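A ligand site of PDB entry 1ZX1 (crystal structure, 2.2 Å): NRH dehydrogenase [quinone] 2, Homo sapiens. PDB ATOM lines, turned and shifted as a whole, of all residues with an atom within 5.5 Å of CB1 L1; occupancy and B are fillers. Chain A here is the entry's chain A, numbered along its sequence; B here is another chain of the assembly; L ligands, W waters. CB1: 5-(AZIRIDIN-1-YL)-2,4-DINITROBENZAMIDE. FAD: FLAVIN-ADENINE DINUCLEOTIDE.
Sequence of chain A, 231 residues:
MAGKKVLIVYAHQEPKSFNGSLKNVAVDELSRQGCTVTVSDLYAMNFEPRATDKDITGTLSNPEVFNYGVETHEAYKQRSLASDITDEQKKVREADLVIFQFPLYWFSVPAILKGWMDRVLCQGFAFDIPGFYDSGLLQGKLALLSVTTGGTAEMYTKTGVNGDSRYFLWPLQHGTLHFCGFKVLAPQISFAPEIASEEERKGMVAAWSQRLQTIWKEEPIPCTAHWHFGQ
The side-chain amide nitrogen of Asn 162 sits at hydrogen-bond distance from an oxygen (O2) of CB1 L1.
The backbone carbonyl oxygen (O) of Gly 150 sits at hydrogen-bond distance from a nitrogen (N1) of CB1 L1 (3.5 Å).
The backbone NH of Trp 106 lies within hydrogen-bond range of a nitrogen (N5) of FAD L2 (2.8 Å).
An oxygen (O2) of FAD L2 lies within hydrogen-bond range of the backbone NH of Gly 151 (3.1 Å).
The backbone NH of Gly 150 sits at hydrogen-bond distance from a nitrogen (N1) of FAD L2 (3.1 Å).
N of Phe 107 lies within hydrogen-bond range of O4 of FAD L2 (2.9 Å).
An oxygen (O2) of FAD L2 is in hydrogen-bond range of the side-chain hydroxyl of Tyr 156.
N of Asn 162 sits at hydrogen-bond distance from O of Met 155 (3.0 Å).
The side-chain amide oxygen (OD1) of Asn 162 sits at hydrogen-bond distance from the side-chain hydroxyl (OH) of Tyr 133 of chain B (2.8 Å).
O of Phe 179 of chain B is in hydrogen-bond range of N of Tyr 133 of chain B.
The backbone NH of Met 155 sits at hydrogen-bond distance from the side-chain hydroxyl of Thr 152 (3.4 Å).
An oxygen (O) of CB1 L1 sits close to the side-chain sulfur (SD) of Met 155, 3.6 Å away.
Merely in contact with CB1 L1: Trp 106 (3.1 Å), Phe 107 (3.8 Å), Gly 151 (3.3 Å), Tyr 156 (3.997 Å), Phe 127 of chain B (3.5 Å) and Phe 179 of chain B (3.4 Å).
Along chain A the residues within 4 Å of CB1 L1 span positions 106 to 162.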
ATOM      1  N   TRP A 106       8.540  18.746 -23.357  1.00  0.00           N
ATOM      2  CA  TRP A 106       9.928  18.738 -23.855  1.00  0.00           C
ATOM      3  C   TRP A 106      10.608  17.341 -23.779  1.00  0.00           C
ATOM      4  O   TRP A 106      11.697  17.180 -23.179  1.00  0.00           O
ATOM      5  CB  TRP A 106      10.740  19.788 -23.103  1.00  0.00           C
ATOM      6  CG  TRP A 106      10.239  21.162 -23.391  1.00  0.00           C
ATOM      7  CD1 TRP A 106       9.752  22.049 -22.509  1.00  0.00           C
ATOM      8  CD2 TRP A 106      10.109  21.762 -24.687  1.00  0.00           C
ATOM      9  NE1 TRP A 106       9.371  23.221 -23.166  1.00  0.00           N
ATOM     10  CE2 TRP A 106       9.593  23.064 -24.511  1.00  0.00           C
ATOM     11  CE3 TRP A 106      10.413  21.331 -25.991  1.00  0.00           C
ATOM     12  CZ2 TRP A 106       9.353  23.930 -25.575  1.00  0.00           C
ATOM     13  CZ3 TRP A 106      10.209  22.204 -27.064  1.00  0.00           C
ATOM     14  CH2 TRP A 106       9.677  23.494 -26.844  1.00  0.00           C
ATOM     15  N   PHE A 107       9.942  16.348 -24.364  1.00  0.00           N
ATOM     16  CA  PHE A 107      10.454  14.976 -24.478  1.00  0.00           C
ATOM     17  C   PHE A 107      10.722  14.360 -23.113  1.00  0.00           C
ATOM     18  O   PHE A 107      11.593  13.516 -22.988  1.00  0.00           O
ATOM     19  CB  PHE A 107      11.757  14.945 -25.304  1.00  0.00           C
ATOM     20  CG  PHE A 107      11.572  14.864 -26.796  1.00  0.00           C
ATOM     21  CD1 PHE A 107      10.548  15.575 -27.436  1.00  0.00           C
ATOM     22  CD2 PHE A 107      12.499  14.147 -27.584  1.00  0.00           C
ATOM     23  CE1 PHE A 107      10.411  15.511 -28.848  1.00  0.00           C
ATOM     24  CE2 PHE A 107      12.390  14.073 -28.990  1.00  0.00           C
ATOM     25  CZ  PHE A 107      11.346  14.762 -29.622  1.00  0.00           C
ATOM     26  N   GLY A 150       1.698  15.554 -27.736  1.00  0.00           N
ATOM     27  CA  GLY A 150       1.087  16.461 -28.706  1.00  0.00           C
ATOM     28  C   GLY A 150       1.299  15.919 -30.112  1.00  0.00           C
ATOM     29  O   GLY A 150       0.423  16.009 -30.964  1.00  0.00           O
ATOM     30  N   GLY A 151       2.474  15.346 -30.346  1.00  0.00           N
ATOM     31  CA  GLY A 151       2.821  14.731 -31.620  1.00  0.00           C
ATOM     32  C   GLY A 151       2.157  13.383 -31.883  1.00  0.00           C
ATOM     33  O   GLY A 151       1.928  12.591 -30.977  1.00  0.00           O
ATOM     34  N   THR A 152       1.858  13.165 -33.165  1.00  0.00           N
ATOM     35  CA  THR A 152       1.267  11.923 -33.666  1.00  0.00           C
ATOM     36  C   THR A 152       2.280  10.779 -33.609  1.00  0.00           C
ATOM     37  O   THR A 152       3.495  11.040 -33.476  1.00  0.00           O
ATOM     38  CB  THR A 152       0.852  12.087 -35.116  1.00  0.00           C
ATOM     39  OG1 THR A 152       1.999  12.485 -35.870  1.00  0.00           O
ATOM     40  CG2 THR A 152      -0.258  13.146 -35.258  1.00  0.00           C
ATOM     41  N   MET A 155       5.034  10.930 -36.168  1.00  0.00           N
ATOM     42  CA  MET A 155       6.128  11.853 -35.833  1.00  0.00           C
ATOM     43  C   MET A 155       7.174  11.178 -34.944  1.00  0.00           C
ATOM     44  O   MET A 155       8.375  11.458 -35.045  1.00  0.00           O
ATOM     45  CB  MET A 155       5.608  13.114 -35.158  1.00  0.00           C
ATOM     46  CG  MET A 155       5.071  14.146 -36.140  1.00  0.00           C
ATOM     47  SD  MET A 155       3.999  15.344 -35.303  1.00  0.00           S
ATOM     48  CE  MET A 155       2.842  15.707 -36.663  1.00  0.00           C
ATOM     49  N   TYR A 156       6.715  10.264 -34.096  1.00  0.00           N
ATOM     50  CA  TYR A 156       7.599   9.493 -33.219  1.00  0.00           C
ATOM     51  C   TYR A 156       8.071   8.154 -33.808  1.00  0.00           C
ATOM     52  O   TYR A 156       8.048   7.139 -33.125  1.00  0.00           O
ATOM     53  CB  TYR A 156       6.971   9.273 -31.844  1.00  0.00           C
ATOM     54  CG  TYR A 156       6.922  10.534 -31.036  1.00  0.00           C
ATOM     55  CD1 TYR A 156       8.059  10.987 -30.351  1.00  0.00           C
ATOM     56  CD2 TYR A 156       5.746  11.305 -30.983  1.00  0.00           C
ATOM     57  CE1 TYR A 156       8.027  12.168 -29.599  1.00  0.00           C
ATOM     58  CE2 TYR A 156       5.693  12.482 -30.254  1.00  0.00           C
ATOM     59  CZ  TYR A 156       6.832  12.912 -29.550  1.00  0.00           C
ATOM     60  OH  TYR A 156       6.797  14.082 -28.833  1.00  0.00           O
ATOM     61  N   VAL A 161      10.205  13.289 -37.788  1.00  0.00           N
ATOM     62  CA  VAL A 161      10.824  14.474 -37.113  1.00  0.00           C
ATOM     63  C   VAL A 161      11.289  14.278 -35.662  1.00  0.00           C
ATOM     64  O   VAL A 161      12.364  14.735 -35.290  1.00  0.00           O
ATOM     65  CB  VAL A 161       9.950  15.773 -37.171  1.00  0.00           C
ATOM     66  CG1 VAL A 161       9.771  16.230 -38.623  1.00  0.00           C
ATOM     67  CG2 VAL A 161       8.539  15.577 -36.420  1.00  0.00           C
ATOM     68  N   ASN A 162      10.478  13.624 -34.839  1.00  0.00           N
ATOM     69  CA  ASN A 162      10.816  13.489 -33.421  1.00  0.00           C
ATOM     70  C   ASN A 162      11.744  12.317 -33.061  1.00  0.00           C
ATOM     71  O   ASN A 162      12.244  12.241 -31.940  1.00  0.00           O
ATOM     72  CB  ASN A 162       9.558  13.404 -32.534  1.00  0.00           C
ATOM     73  CG  ASN A 162       8.746  14.691 -32.513  1.00  0.00           C
ATOM     74  OD1 ASN A 162       9.267  15.804 -32.679  1.00  0.00           O
ATOM     75  ND2 ASN A 162       7.437  14.543 -32.259  1.00  0.00           N
ATOM     76  N   ILE A 195      -5.759  16.226 -30.946  1.00  0.00           N
ATOM     77  CA  ILE A 195      -6.030  16.131 -32.389  1.00  0.00           C
ATOM     78  C   ILE A 195      -7.028  15.009 -32.717  1.00  0.00           C
ATOM     79  O   ILE A 195      -7.814  15.125 -33.653  1.00  0.00           O
ATOM     80  CB  ILE A 195      -4.701  15.917 -33.187  1.00  0.00           C
ATOM     81  CG1 ILE A 195      -4.100  17.250 -33.578  1.00  0.00           C
ATOM     82  CG2 ILE A 195      -4.925  15.123 -34.456  1.00  0.00           C
ATOM     83  CD1 ILE A 195      -2.570  17.188 -33.735  1.00  0.00           C
ATOM     84  N   GLN B 123       4.838  28.557 -26.975  1.00  0.00           N
ATOM     85  CA  GLN B 123       4.403  28.705 -28.334  1.00  0.00           C
ATOM     86  C   GLN B 123       4.191  30.179 -28.660  1.00  0.00           C
ATOM     87  O   GLN B 123       3.666  30.947 -27.844  1.00  0.00           O
ATOM     88  CB  GLN B 123       3.094  27.937 -28.532  1.00  0.00           C
ATOM     89  CG  GLN B 123       2.749  27.794 -30.021  1.00  0.00           C
ATOM     90  CD  GLN B 123       1.590  26.886 -30.258  1.00  0.00           C
ATOM     91  OE1 GLN B 123       1.162  26.169 -29.341  1.00  0.00           O
ATOM     92  NE2 GLN B 123       1.091  26.859 -31.488  1.00  0.00           N
ATOM     93  N   PHE B 127       8.700  28.613 -30.582  1.00  0.00           N
ATOM     94  CA  PHE B 127       8.319  27.812 -31.702  1.00  0.00           C
ATOM     95  C   PHE B 127       6.897  28.191 -32.029  1.00  0.00           C
ATOM     96  O   PHE B 127       6.204  28.851 -31.235  1.00  0.00           O
ATOM     97  CB  PHE B 127       8.366  26.331 -31.350  1.00  0.00           C
ATOM     98  CG  PHE B 127       7.316  25.911 -30.389  1.00  0.00           C
ATOM     99  CD1 PHE B 127       7.500  26.084 -29.023  1.00  0.00           C
ATOM    100  CD2 PHE B 127       6.146  25.326 -30.840  1.00  0.00           C
ATOM    101  CE1 PHE B 127       6.528  25.695 -28.125  1.00  0.00           C
ATOM    102  CE2 PHE B 127       5.144  24.932 -29.949  1.00  0.00           C
ATOM    103  CZ  PHE B 127       5.330  25.128 -28.593  1.00  0.00           C
ATOM    104  N   ILE B 129       3.395  26.187 -34.348  1.00  0.00           N
ATOM    105  CA  ILE B 129       2.885  25.002 -35.016  1.00  0.00           C
ATOM    106  C   ILE B 129       2.106  25.514 -36.191  1.00  0.00           C
ATOM    107  O   ILE B 129       0.930  25.903 -36.029  1.00  0.00           O
ATOM    108  CB  ILE B 129       1.962  24.154 -34.121  1.00  0.00           C
ATOM    109  CG1 ILE B 129       2.702  23.684 -32.859  1.00  0.00           C
ATOM    110  CG2 ILE B 129       1.353  22.968 -34.919  1.00  0.00           C
ATOM    111  CD1 ILE B 129       4.001  22.929 -33.122  1.00  0.00           C
ATOM    112  N   TYR B 133      11.868  22.924 -35.147  1.00  0.00           N
ATOM    113  CA  TYR B 133      13.184  22.425 -35.617  1.00  0.00           C
ATOM    114  C   TYR B 133      13.881  23.489 -36.465  1.00  0.00           C
ATOM    115  O   TYR B 133      14.059  24.602 -35.998  1.00  0.00           O
ATOM    116  CB  TYR B 133      13.076  21.041 -36.316  1.00  0.00           C
ATOM    117  CG  TYR B 133      12.733  19.942 -35.341  1.00  0.00           C
ATOM    118  CD1 TYR B 133      13.571  19.659 -34.273  1.00  0.00           C
ATOM    119  CD2 TYR B 133      11.571  19.182 -35.497  1.00  0.00           C
ATOM    120  CE1 TYR B 133      13.253  18.680 -33.366  1.00  0.00           C
ATOM    121  CE2 TYR B 133      11.257  18.174 -34.584  1.00  0.00           C
ATOM    122  CZ  TYR B 133      12.116  17.946 -33.508  1.00  0.00           C
ATOM    123  OH  TYR B 133      11.838  16.963 -32.590  1.00  0.00           O
ATOM    124  N   GLY B 175      15.023  17.418 -28.653  1.00  0.00           N
ATOM    125  CA  GLY B 175      13.631  17.594 -28.315  1.00  0.00           C
ATOM    126  C   GLY B 175      13.296  19.016 -27.912  1.00  0.00           C
ATOM    127  O   GLY B 175      12.165  19.463 -28.107  1.00  0.00           O
ATOM    128  N   PHE B 179      14.439  21.771 -31.542  1.00  0.00           N
ATOM    129  CA  PHE B 179      13.012  22.011 -31.769  1.00  0.00           C
ATOM    130  C   PHE B 179      12.745  23.524 -31.836  1.00  0.00           C
ATOM    131  O   PHE B 179      11.975  23.977 -32.674  1.00  0.00           O
ATOM    132  CB  PHE B 179      12.119  21.345 -30.666  1.00  0.00           C
ATOM    133  CG  PHE B 179      10.629  21.466 -30.944  1.00  0.00           C
ATOM    134  CD1 PHE B 179       9.932  20.468 -31.652  1.00  0.00           C
ATOM    135  CD2 PHE B 179       9.904  22.581 -30.509  1.00  0.00           C
ATOM    136  CE1 PHE B 179       8.536  20.598 -31.937  1.00  0.00           C
ATOM    137  CE2 PHE B 179       8.525  22.716 -30.780  1.00  0.00           C
ATOM    138  CZ  PHE B 179       7.846  21.711 -31.499  1.00  0.00           C
HETATM  139  C   CB1 L   1       6.140  19.445 -29.207  1.00  0.00           C
HETATM  140  C1  CB1 L   1       5.556  18.742 -30.265  1.00  0.00           C
HETATM  141  C2  CB1 L   1       4.241  19.071 -30.650  1.00  0.00           C
HETATM  142  C4  CB1 L   1       3.564  20.084 -29.965  1.00  0.00           C
HETATM  143  C5  CB1 L   1       4.147  20.787 -28.908  1.00  0.00           C
HETATM  144  C8  CB1 L   1       5.457  20.465 -28.519  1.00  0.00           C
HETATM  145  N   CB1 L   1       6.311  17.792 -30.857  1.00  0.00           N
HETATM  146  O1  CB1 L   1       7.713  17.614 -30.465  1.00  0.00           O
HETATM  147  O2  CB1 L   1       5.821  16.913 -31.855  1.00  0.00           O
HETATM  148  C3  CB1 L   1       3.482  18.410 -31.797  1.00  0.00           C
HETATM  149  N1  CB1 L   1       2.217  18.805 -31.968  1.00  0.00           N
HETATM  150  O   CB1 L   1       4.024  17.620 -32.556  1.00  0.00           O
HETATM  151  N6  CB1 L   1       3.484  21.763 -28.284  1.00  0.00           N
HETATM  152  C7  CB1 L   1       2.325  22.329 -29.029  1.00  0.00           C
HETATM  153  C9  CB1 L   1       2.121  21.463 -27.787  1.00  0.00           C
HETATM  154  N3  CB1 L   1       6.084  21.124 -27.540  1.00  0.00           N
HETATM  155  O3  CB1 L   1       7.412  20.842 -27.260  1.00  0.00           O
HETATM  156  O4  CB1 L   1       5.519  22.145 -26.791  1.00  0.00           O
HETATM  157  PA  FAD L   2      -6.540  17.555 -23.054  1.00  0.00           P
HETATM  158  O1A FAD L   2      -6.389  18.761 -23.994  1.00  0.00           O
HETATM  159  O2A FAD L   2      -7.015  18.010 -21.693  1.00  0.00           O
HETATM  160  O5B FAD L   2      -7.642  16.579 -23.684  1.00  0.00           O
HETATM  161  C5B FAD L   2      -7.709  16.374 -25.076  1.00  0.00           C
HETATM  162  C4B FAD L   2      -9.204  16.345 -25.350  1.00  0.00           C
HETATM  163  O4B FAD L   2      -9.751  15.175 -24.780  1.00  0.00           O
HETATM  164  C3B FAD L   2      -9.895  17.547 -24.688  1.00  0.00           C
HETATM  165  O3B FAD L   2     -10.586  18.270 -25.697  1.00  0.00           O
HETATM  166  C2B FAD L   2     -10.816  16.936 -23.619  1.00  0.00           C
HETATM  167  O2B FAD L   2     -12.077  17.576 -23.489  1.00  0.00           O
HETATM  168  C1B FAD L   2     -10.973  15.504 -24.122  1.00  0.00           C
HETATM  169  N9A FAD L   2     -11.298  14.478 -23.101  1.00  0.00           N
HETATM  170  C8A FAD L   2     -11.050  14.490 -21.738  1.00  0.00           C
HETATM  171  N7A FAD L   2     -11.528  13.336 -21.218  1.00  0.00           N
HETATM  172  C5A FAD L   2     -12.072  12.575 -22.224  1.00  0.00           C
HETATM  173  C6A FAD L   2     -12.704  11.313 -22.261  1.00  0.00           C
HETATM  174  N6A FAD L   2     -13.121  10.738 -21.143  1.00  0.00           N
HETATM  175  N1A FAD L   2     -13.166  10.820 -23.475  1.00  0.00           N
HETATM  176  C2A FAD L   2     -13.013  11.552 -24.638  1.00  0.00           C
HETATM  177  N3A FAD L   2     -12.395  12.799 -24.595  1.00  0.00           N
HETATM  178  C4A FAD L   2     -11.930  13.295 -23.405  1.00  0.00           C
HETATM  179  N1  FAD L   2       4.177  17.219 -26.947  1.00  0.00           N
HETATM  180  C2  FAD L   2       5.129  16.442 -27.536  1.00  0.00           C
HETATM  181  O2  FAD L   2       4.780  15.568 -28.335  1.00  0.00           O
HETATM  182  N3  FAD L   2       6.474  16.612 -27.294  1.00  0.00           N
HETATM  183  C4  FAD L   2       6.914  17.549 -26.410  1.00  0.00           C
HETATM  184  O4  FAD L   2       8.120  17.635 -26.239  1.00  0.00           O
HETATM  185  C4X FAD L   2       5.964  18.388 -25.802  1.00  0.00           C
HETATM  186  N5  FAD L   2       6.371  19.402 -24.946  1.00  0.00           N
HETATM  187  C5X FAD L   2       5.405  20.185 -24.337  1.00  0.00           C
HETATM  188  C6  FAD L   2       5.831  21.179 -23.448  1.00  0.00           C
HETATM  189  C7  FAD L   2       4.910  21.983 -22.791  1.00  0.00           C
HETATM  190  C7M FAD L   2       5.450  23.021 -21.846  1.00  0.00           C
HETATM  191  C8  FAD L   2       3.537  21.803 -23.053  1.00  0.00           C
HETATM  192  C8M FAD L   2       2.480  22.638 -22.418  1.00  0.00           C
HETATM  193  C9  FAD L   2       3.106  20.803 -23.963  1.00  0.00           C
HETATM  194  C9A FAD L   2       4.018  19.977 -24.595  1.00  0.00           C
HETATM  195  N10 FAD L   2       3.628  18.973 -25.493  1.00  0.00           N
HETATM  196  C10 FAD L   2       4.604  18.203 -26.084  1.00  0.00           C
HETATM  197  C1' FAD L   2       2.178  18.607 -25.831  1.00  0.00           C
HETATM  198  C2' FAD L   2       1.522  17.834 -24.661  1.00  0.00           C
HETATM  199  O2' FAD L   2       2.217  16.628 -24.391  1.00  0.00           O
HETATM  200  C3' FAD L   2       0.029  17.676 -24.931  1.00  0.00           C
HETATM  201  O3' FAD L   2      -0.558  18.962 -24.960  1.00  0.00           O
HETATM  202  C4' FAD L   2      -0.698  16.821 -23.883  1.00  0.00           C
HETATM  203  O4' FAD L   2      -0.142  15.527 -23.837  1.00  0.00           O
HETATM  204  C5' FAD L   2      -2.165  16.612 -24.222  1.00  0.00           C
HETATM  205  O5' FAD L   2      -2.758  15.868 -23.155  1.00  0.00           O
HETATM  206  P   FAD L   2      -3.905  16.519 -22.225  1.00  0.00           P
HETATM  207  O1P FAD L   2      -3.324  17.834 -21.742  1.00  0.00           O
HETATM  208  O2P FAD L   2      -4.266  15.622 -21.070  1.00  0.00           O
HETATM  209  O3P FAD L   2      -5.179  16.661 -23.199  1.00  0.00           O
HETATM  210  O   HOH W   1       9.631  18.583 -28.621  1.00  0.00           O
